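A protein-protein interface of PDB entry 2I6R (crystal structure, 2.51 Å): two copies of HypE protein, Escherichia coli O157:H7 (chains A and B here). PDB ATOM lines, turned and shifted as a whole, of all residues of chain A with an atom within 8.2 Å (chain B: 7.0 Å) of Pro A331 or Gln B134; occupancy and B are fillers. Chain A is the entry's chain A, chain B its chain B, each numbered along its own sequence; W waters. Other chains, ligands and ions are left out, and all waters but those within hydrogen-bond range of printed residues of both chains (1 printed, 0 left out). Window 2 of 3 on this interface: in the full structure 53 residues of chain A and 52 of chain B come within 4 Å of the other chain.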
ATOM      1  N   VAL A  59      17.287   4.036  17.825  1.00  0.00           N
ATOM      2  CA  VAL A  59      16.856   5.005  16.812  1.00  0.00           C
ATOM      3  C   VAL A  59      17.988   5.979  16.465  1.00  0.00           C
ATOM      4  O   VAL A  59      17.754   7.087  15.968  1.00  0.00           O
ATOM      5  CB  VAL A  59      15.606   5.799  17.287  1.00  0.00           C
ATOM      6  CG1 VAL A  59      14.385   4.872  17.457  1.00  0.00           C
ATOM      7  CG2 VAL A  59      15.897   6.577  18.593  1.00  0.00           C
ATOM      8  N   ILE A  60      19.216   5.546  16.724  1.00  0.00           N
ATOM      9  CA  ILE A  60      20.393   6.383  16.543  1.00  0.00           C
ATOM     10  C   ILE A  60      20.523   6.963  15.124  1.00  0.00           C
ATOM     11  O   ILE A  60      20.258   6.287  14.135  1.00  0.00           O
ATOM     12  CB  ILE A  60      21.695   5.630  16.973  1.00  0.00           C
ATOM     13  CG1 ILE A  60      22.890   6.585  17.042  1.00  0.00           C
ATOM     14  CG2 ILE A  60      21.970   4.421  16.059  1.00  0.00           C
ATOM     15  CD1 ILE A  60      24.070   6.027  17.788  1.00  0.00           C
ATOM     16  N   ASP A  61      20.911   8.230  15.053  1.00  0.00           N
ATOM     17  CA  ASP A  61      21.204   8.907  13.797  1.00  0.00           C
ATOM     18  C   ASP A  61      22.611   9.470  13.985  1.00  0.00           C
ATOM     19  O   ASP A  61      22.843  10.218  14.938  1.00  0.00           O
ATOM     20  CB  ASP A  61      20.168  10.017  13.570  1.00  0.00           C
ATOM     21  CG  ASP A  61      20.433  10.857  12.328  1.00  0.00           C
ATOM     22  OD1 ASP A  61      20.510  12.091  12.485  1.00  0.00           O
ATOM     23  OD2 ASP A  61      20.534  10.315  11.203  1.00  0.00           O
ATOM     24  N   PRO A  62      23.571   9.072  13.123  1.00  0.00           N
ATOM     25  CA  PRO A  62      23.410   8.191  11.964  1.00  0.00           C
ATOM     26  C   PRO A  62      23.607   6.706  12.298  1.00  0.00           C
ATOM     27  O   PRO A  62      23.942   6.353  13.432  1.00  0.00           O
ATOM     28  CB  PRO A  62      24.507   8.679  11.007  1.00  0.00           C
ATOM     29  CG  PRO A  62      25.585   9.263  11.908  1.00  0.00           C
ATOM     30  CD  PRO A  62      24.978   9.494  13.280  1.00  0.00           C
ATOM     31  N   GLY A 136       9.290   8.462   4.172  1.00  0.00           N
ATOM     32  CA  GLY A 136       8.852   9.562   5.015  1.00  0.00           C
ATOM     33  C   GLY A 136       8.305   9.134   6.361  1.00  0.00           C
ATOM     34  O   GLY A 136       8.333   9.923   7.308  1.00  0.00           O
ATOM     35  N   ASP A 139      12.794   7.170   9.568  1.00  0.00           N
ATOM     36  CA  ASP A 139      14.106   7.584   9.129  1.00  0.00           C
ATOM     37  C   ASP A 139      14.983   6.346   9.004  1.00  0.00           C
ATOM     38  O   ASP A 139      15.642   5.937   9.961  1.00  0.00           O
ATOM     39  CB  ASP A 139      14.696   8.595  10.106  1.00  0.00           C
ATOM     40  CG  ASP A 139      15.942   9.281   9.564  1.00  0.00           C
ATOM     41  OD1 ASP A 139      16.196   9.211   8.337  1.00  0.00           O
ATOM     42  OD2 ASP A 139      16.670   9.895  10.377  1.00  0.00           O
ATOM     43  N   PHE A 142      14.788   1.558  12.382  1.00  0.00           N
ATOM     44  CA  PHE A 142      14.752   1.438  13.847  1.00  0.00           C
ATOM     45  C   PHE A 142      14.777  -0.036  14.260  1.00  0.00           C
ATOM     46  O   PHE A 142      14.211  -0.883  13.573  1.00  0.00           O
ATOM     47  CB  PHE A 142      13.499   2.080  14.450  1.00  0.00           C
ATOM     48  CG  PHE A 142      13.245   3.491  14.022  1.00  0.00           C
ATOM     49  CD1 PHE A 142      14.275   4.427  13.960  1.00  0.00           C
ATOM     50  CD2 PHE A 142      11.951   3.899  13.719  1.00  0.00           C
ATOM     51  CE1 PHE A 142      14.025   5.745  13.572  1.00  0.00           C
ATOM     52  CE2 PHE A 142      11.685   5.212  13.335  1.00  0.00           C
ATOM     53  CZ  PHE A 142      12.724   6.140  13.260  1.00  0.00           C
ATOM     54  N   ILE A 181      28.827  11.038  18.733  1.00  0.00           N
ATOM     55  CA  ILE A 181      27.617  11.268  17.963  1.00  0.00           C
ATOM     56  C   ILE A 181      27.370  12.764  17.803  1.00  0.00           C
ATOM     57  O   ILE A 181      27.061  13.235  16.707  1.00  0.00           O
ATOM     58  CB  ILE A 181      26.396  10.559  18.600  1.00  0.00           C
ATOM     59  CG1 ILE A 181      26.652   9.050  18.773  1.00  0.00           C
ATOM     60  CG2 ILE A 181      25.118  10.826  17.797  1.00  0.00           C
ATOM     61  CD1 ILE A 181      27.261   8.318  17.560  1.00  0.00           C
ATOM     62  N   LEU A 182      27.528  13.508  18.891  1.00  0.00           N
ATOM     63  CA  LEU A 182      27.431  14.960  18.849  1.00  0.00           C
ATOM     64  C   LEU A 182      28.301  15.534  17.735  1.00  0.00           C
ATOM     65  O   LEU A 182      27.826  16.300  16.901  1.00  0.00           O
ATOM     66  CB  LEU A 182      27.865  15.556  20.184  1.00  0.00           C
ATOM     67  CG  LEU A 182      26.825  15.673  21.292  1.00  0.00           C
ATOM     68  CD1 LEU A 182      27.495  15.542  22.653  1.00  0.00           C
ATOM     69  CD2 LEU A 182      26.085  17.010  21.174  1.00  0.00           C
ATOM     70  N   ARG A 185      26.936  14.820  14.104  1.00  0.00           N
ATOM     71  CA  ARG A 185      25.721  15.571  13.811  1.00  0.00           C
ATOM     72  C   ARG A 185      25.966  17.080  13.738  1.00  0.00           C
ATOM     73  O   ARG A 185      25.228  17.794  13.055  1.00  0.00           O
ATOM     74  CB  ARG A 185      24.640  15.249  14.846  1.00  0.00           C
ATOM     75  CG  ARG A 185      24.368  13.759  14.997  1.00  0.00           C
ATOM     76  CD  ARG A 185      23.053  13.349  14.384  1.00  0.00           C
ATOM     77  NE  ARG A 185      22.045  13.160  15.427  1.00  0.00           N
ATOM     78  CZ  ARG A 185      21.068  14.020  15.688  1.00  0.00           C
ATOM     79  NH1 ARG A 185      20.946  15.140  14.977  1.00  0.00           N
ATOM     80  NH2 ARG A 185      20.213  13.758  16.661  1.00  0.00           N
ATOM     81  N   ARG A 222      21.309   6.503  28.351  1.00  0.00           N
ATOM     82  CA  ARG A 222      20.590   7.781  28.346  1.00  0.00           C
ATOM     83  C   ARG A 222      20.709   8.461  29.709  1.00  0.00           C
ATOM     84  O   ARG A 222      20.455   7.840  30.738  1.00  0.00           O
ATOM     85  CB  ARG A 222      19.112   7.573  27.973  1.00  0.00           C
ATOM     86  CG  ARG A 222      18.232   8.797  28.206  1.00  0.00           C
ATOM     87  CD  ARG A 222      16.762   8.522  27.905  1.00  0.00           C
ATOM     88  NE  ARG A 222      15.960   9.757  27.803  1.00  0.00           N
ATOM     89  CZ  ARG A 222      16.333  10.890  27.188  1.00  0.00           C
ATOM     90  NH1 ARG A 222      17.513  10.986  26.571  1.00  0.00           N
ATOM     91  NH2 ARG A 222      15.511  11.940  27.181  1.00  0.00           N
ATOM     92  N   PRO A 329      18.848  17.704  25.839  1.00  0.00           N
ATOM     93  CA  PRO A 329      19.714  16.687  25.229  1.00  0.00           C
ATOM     94  C   PRO A 329      19.362  16.428  23.759  1.00  0.00           C
ATOM     95  O   PRO A 329      18.171  16.349  23.402  1.00  0.00           O
ATOM     96  CB  PRO A 329      19.455  15.433  26.077  1.00  0.00           C
ATOM     97  CG  PRO A 329      18.099  15.636  26.680  1.00  0.00           C
ATOM     98  CD  PRO A 329      17.762  17.117  26.646  1.00  0.00           C
ATOM     99  N   LEU A 330      20.394  16.315  22.916  1.00  0.00           N
ATOM    100  CA  LEU A 330      20.198  16.053  21.484  1.00  0.00           C
ATOM    101  C   LEU A 330      19.471  14.725  21.304  1.00  0.00           C
ATOM    102  O   LEU A 330      19.846  13.722  21.921  1.00  0.00           O
ATOM    103  CB  LEU A 330      21.530  16.046  20.722  1.00  0.00           C
ATOM    104  CG  LEU A 330      21.471  16.197  19.197  1.00  0.00           C
ATOM    105  CD1 LEU A 330      21.345  17.669  18.785  1.00  0.00           C
ATOM    106  CD2 LEU A 330      22.686  15.562  18.533  1.00  0.00           C
ATOM    107  N   PRO A 331      18.397  14.726  20.494  1.00  0.00           N
ATOM    108  CA  PRO A 331      17.650  13.487  20.255  1.00  0.00           C
ATOM    109  C   PRO A 331      18.454  12.451  19.468  1.00  0.00           C
ATOM    110  O   PRO A 331      19.443  12.793  18.819  1.00  0.00           O
ATOM    111  CB  PRO A 331      16.428  13.961  19.452  1.00  0.00           C
ATOM    112  CG  PRO A 331      16.828  15.279  18.858  1.00  0.00           C
ATOM    113  CD  PRO A 331      17.810  15.889  19.794  1.00  0.00           C
ATOM    114  N   ARG A 332      18.038  11.188  19.564  1.00  0.00           N
ATOM    115  CA  ARG A 332      18.592  10.101  18.749  1.00  0.00           C
ATOM    116  C   ARG A 332      20.102   9.850  18.898  1.00  0.00           C
ATOM    117  O   ARG A 332      20.783   9.545  17.920  1.00  0.00           O
ATOM    118  CB  ARG A 332      18.205  10.302  17.280  1.00  0.00           C
ATOM    119  CG  ARG A 332      16.706  10.375  17.086  1.00  0.00           C
ATOM    120  CD  ARG A 332      16.306  10.439  15.640  1.00  0.00           C
ATOM    121  NE  ARG A 332      16.778   9.314  14.837  1.00  0.00           N
ATOM    122  CZ  ARG A 332      16.656   9.251  13.516  1.00  0.00           C
ATOM    123  NH1 ARG A 332      16.061  10.241  12.862  1.00  0.00           N
ATOM    124  NH2 ARG A 332      17.119   8.202  12.847  1.00  0.00           N
ATOM    125  N   ILE A 333      20.615   9.980  20.118  1.00  0.00           N
ATOM    126  CA  ILE A 333      22.020   9.647  20.401  1.00  0.00           C
ATOM    127  C   ILE A 333      22.164   8.134  20.616  1.00  0.00           C
ATOM    128  O   ILE A 333      23.216   7.556  20.351  1.00  0.00           O
ATOM    129  CB  ILE A 333      22.609  10.512  21.567  1.00  0.00           C
ATOM    130  CG1 ILE A 333      23.084  11.862  21.016  1.00  0.00           C
ATOM    131  CG2 ILE A 333      23.761   9.804  22.282  1.00  0.00           C
ATOM    132  CD1 ILE A 333      23.450  12.911  22.087  1.00  0.00           C
ATOM    133  N   CYS A 334      21.085   7.510  21.081  1.00  0.00           N
ATOM    134  CA  CYS A 334      20.948   6.050  21.097  1.00  0.00           C
ATOM    135  C   CYS A 334      19.666   5.669  20.346  1.00  0.00           C
ATOM    136  O   CYS A 334      19.505   4.547  19.877  1.00  0.00           O
ATOM    137  CB  CYS A 334      20.885   5.527  22.536  1.00  0.00           C
ATOM    138  SG  CYS A 334      21.891   6.475  23.744  1.00  0.00           S
ATOM    139  N   LEU B  98       8.170   7.449  19.579  1.00  0.00           N
ATOM    140  CA  LEU B  98       7.246   8.572  19.441  1.00  0.00           C
ATOM    141  C   LEU B  98       7.810   9.668  18.572  1.00  0.00           C
ATOM    142  O   LEU B  98       8.977  10.046  18.709  1.00  0.00           O
ATOM    143  CB  LEU B  98       6.932   9.195  20.803  1.00  0.00           C
ATOM    144  CG  LEU B  98       6.687   8.315  22.022  1.00  0.00           C
ATOM    145  CD1 LEU B  98       6.680   9.164  23.265  1.00  0.00           C
ATOM    146  CD2 LEU B  98       5.382   7.562  21.888  1.00  0.00           C
ATOM    147  N   GLU B  99       6.962  10.187  17.689  1.00  0.00           N
ATOM    148  CA  GLU B  99       7.231  11.429  16.991  1.00  0.00           C
ATOM    149  C   GLU B  99       6.993  12.576  17.966  1.00  0.00           C
ATOM    150  O   GLU B  99       5.937  12.652  18.592  1.00  0.00           O
ATOM    151  CB  GLU B  99       6.281  11.554  15.808  1.00  0.00           C
ATOM    152  CG  GLU B  99       6.566  12.695  14.848  1.00  0.00           C
ATOM    153  CD  GLU B  99       5.478  12.829  13.784  1.00  0.00           C
ATOM    154  OE1 GLU B  99       5.781  13.316  12.668  1.00  0.00           O
ATOM    155  OE2 GLU B  99       4.316  12.441  14.058  1.00  0.00           O
ATOM    156  N   GLU B 100       7.981  13.458  18.096  1.00  0.00           N
ATOM    157  CA  GLU B 100       7.841  14.674  18.901  1.00  0.00           C
ATOM    158  C   GLU B 100       6.625  15.471  18.422  1.00  0.00           C
ATOM    159  O   GLU B 100       6.346  15.536  17.216  1.00  0.00           O
ATOM    160  CB  GLU B 100       9.113  15.523  18.820  1.00  0.00           C
ATOM    161  CG  GLU B 100       9.602  16.073  20.167  1.00  0.00           C
ATOM    162  CD  GLU B 100       9.109  17.484  20.461  1.00  0.00           C
ATOM    163  OE1 GLU B 100       8.671  18.187  19.515  1.00  0.00           O
ATOM    164  OE2 GLU B 100       9.172  17.894  21.644  1.00  0.00           O
ATOM    165  N   GLY B 101       5.890  16.041  19.380  1.00  0.00           N
ATOM    166  CA  GLY B 101       4.653  16.777  19.091  1.00  0.00           C
ATOM    167  C   GLY B 101       3.418  15.913  18.864  1.00  0.00           C
ATOM    168  O   GLY B 101       2.412  16.394  18.337  1.00  0.00           O
ATOM    169  N   VAL B 132      12.126   9.051  21.669  1.00  0.00           N
ATOM    170  CA  VAL B 132      11.447  10.137  20.974  1.00  0.00           C
ATOM    171  C   VAL B 132      12.322  10.620  19.829  1.00  0.00           C
ATOM    172  O   VAL B 132      13.504  10.911  20.008  1.00  0.00           O
ATOM    173  CB  VAL B 132      11.108  11.327  21.918  1.00  0.00           C
ATOM    174  CG1 VAL B 132      10.487  12.488  21.130  1.00  0.00           C
ATOM    175  CG2 VAL B 132      10.172  10.888  23.048  1.00  0.00           C
ATOM    176  N   VAL B 133      11.730  10.696  18.652  1.00  0.00           N
ATOM    177  CA  VAL B 133      12.406  11.207  17.473  1.00  0.00           C
ATOM    178  C   VAL B 133      11.733  12.505  17.069  1.00  0.00           C
ATOM    179  O   VAL B 133      10.634  12.798  17.530  1.00  0.00           O
ATOM    180  CB  VAL B 133      12.345  10.192  16.318  1.00  0.00           C
ATOM    181  CG1 VAL B 133      13.156   8.944  16.664  1.00  0.00           C
ATOM    182  CG2 VAL B 133      10.885   9.812  15.999  1.00  0.00           C
ATOM    183  N   GLN B 134      12.383  13.285  16.214  1.00  0.00           N
ATOM    184  CA  GLN B 134      11.832  14.572  15.793  1.00  0.00           C
ATOM    185  C   GLN B 134      10.703  14.398  14.783  1.00  0.00           C
ATOM    186  O   GLN B 134      10.466  13.293  14.292  1.00  0.00           O
ATOM    187  CB  GLN B 134      12.924  15.504  15.242  1.00  0.00           C
ATOM    188  CG  GLN B 134      13.829  14.885  14.174  1.00  0.00           C
ATOM    189  CD  GLN B 134      14.991  14.100  14.780  1.00  0.00           C
ATOM    190  OE1 GLN B 134      15.774  14.631  15.585  1.00  0.00           O
ATOM    191  NE2 GLN B 134      15.112  12.836  14.385  1.00  0.00           N
ATOM    192  N   ARG B 135      10.005  15.495  14.498  1.00  0.00           N
ATOM    193  CA  ARG B 135       8.939  15.508  13.503  1.00  0.00           C
ATOM    194  C   ARG B 135       9.468  15.033  12.154  1.00  0.00           C
ATOM    195  O   ARG B 135      10.509  15.502  11.683  1.00  0.00           O
ATOM    196  CB  ARG B 135       8.343  16.915  13.369  1.00  0.00           C
ATOM    197  CG  ARG B 135       7.440  17.313  14.522  1.00  0.00           C
ATOM    198  CD  ARG B 135       6.915  18.737  14.380  1.00  0.00           C
ATOM    199  NE  ARG B 135       6.099  19.127  15.529  1.00  0.00           N
ATOM    200  CZ  ARG B 135       6.589  19.572  16.687  1.00  0.00           C
ATOM    201  NH1 ARG B 135       7.902  19.688  16.864  1.00  0.00           N
ATOM    202  NH2 ARG B 135       5.766  19.898  17.678  1.00  0.00           N
ATOM    203  N   GLY B 136       8.754  14.091  11.549  1.00  0.00           N
ATOM    204  CA  GLY B 136       9.133  13.560  10.248  1.00  0.00           C
ATOM    205  C   GLY B 136      10.039  12.342  10.298  1.00  0.00           C
ATOM    206  O   GLY B 136      10.221  11.662   9.286  1.00  0.00           O
ATOM    207  N   ALA B 137      10.607  12.057  11.465  1.00  0.00           N
ATOM    208  CA  ALA B 137      11.480  10.895  11.613  1.00  0.00           C
ATOM    209  C   ALA B 137      10.701   9.602  11.861  1.00  0.00           C
ATOM    210  O   ALA B 137      11.222   8.510  11.653  1.00  0.00           O
ATOM    211  CB  ALA B 137      12.494  11.133  12.707  1.00  0.00           C
ATOM    212  N   ALA B 138       9.460   9.729  12.320  1.00  0.00           N
ATOM    213  CA  ALA B 138       8.564   8.589  12.525  1.00  0.00           C
ATOM    214  C   ALA B 138       7.140   9.088  12.359  1.00  0.00           C
ATOM    215  O   ALA B 138       6.879  10.271  12.585  1.00  0.00           O
ATOM    216  CB  ALA B 138       8.758   7.974  13.911  1.00  0.00           C
HETATM  217  O   HOH W   1       6.516  10.983   9.633  1.00  0.00           O
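Water W1 bridges the backbone carbonyl oxygen of Ala B138 (3.1 Å) and the backbone carbonyl oxygen of Gly A136 (3.1 Å).
Of the 11 printed residues of chain B, 4 touch a printed residue of chain A. Hydrophobic or aromatic side chains of chain B within 4 Å of the printed part of chain A: Val B133 and Ala B137. Among the printed residues, no Asp or Glu carboxylate lies within 4 Å of a Lys or Arg side-chain nitrogen of the other chain.
O of Gly B136 lies close to O of Gly A136, 3.2 Å away. The backbone carbonyl oxygen of Ala B137 sits at hydrogen-bond distance from the backbone NH of Asp A139, at 2.9 Å. The side-chain amide nitrogen (NE2) of Gln B134 lies close to the guanidinium group (NH1) of Arg A332 (3.2 Å).
Phe A142 touches Ala B137 (CZ to O, 3.2 Å). Pro A331 touches Gln B134. Arg A332 touches Val B133. Ala B137 touches Arg A332 (CB to NH1, 3.7 Å).
Printed residues of chain B within 4 Å of Asp A139: Ala B137. Ile A181 touches none of the printed residues of chain B. Of the printed residues of chain B, Pro A331 touches Gln B134. Gln B134 touches just these residues of chain A: Pro A331 and Arg A332. Of the printed residues of chain A, Gly B136 touches Gly A136.
Gly A136 touches its own counterpart, Gly B136. 1 position is printed for both chains. Of the 7 pairs that touch across the chains among the printed residues, 1 has its exchanged pair printed and touching as well.
The side-chain carboxylate (OE1) of Glu B99 lies within hydrogen-bond range of the backbone NH (N) of Gly B136 (3.3 Å). The backbone carbonyl oxygen of Leu B98 lies within hydrogen-bond range of the backbone NH of Val B133. The backbone carbonyl oxygen of Arg A332 sits at hydrogen-bond distance from the backbone NH of Asp A61 (3.2 Å). NH2 of Arg A185 sits at hydrogen-bond distance from O of Pro A331 (2.5 Å). The side-chain carboxylate (OD2) of Asp A139 is in salt-bridge range of the guanidinium group (NH1) of Arg A332 (2.6 Å). The backbone NH (N) of Glu B100 sits at hydrogen-bond distance from the backbone carbonyl oxygen (O) of Val B133, 2.8 Å away.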
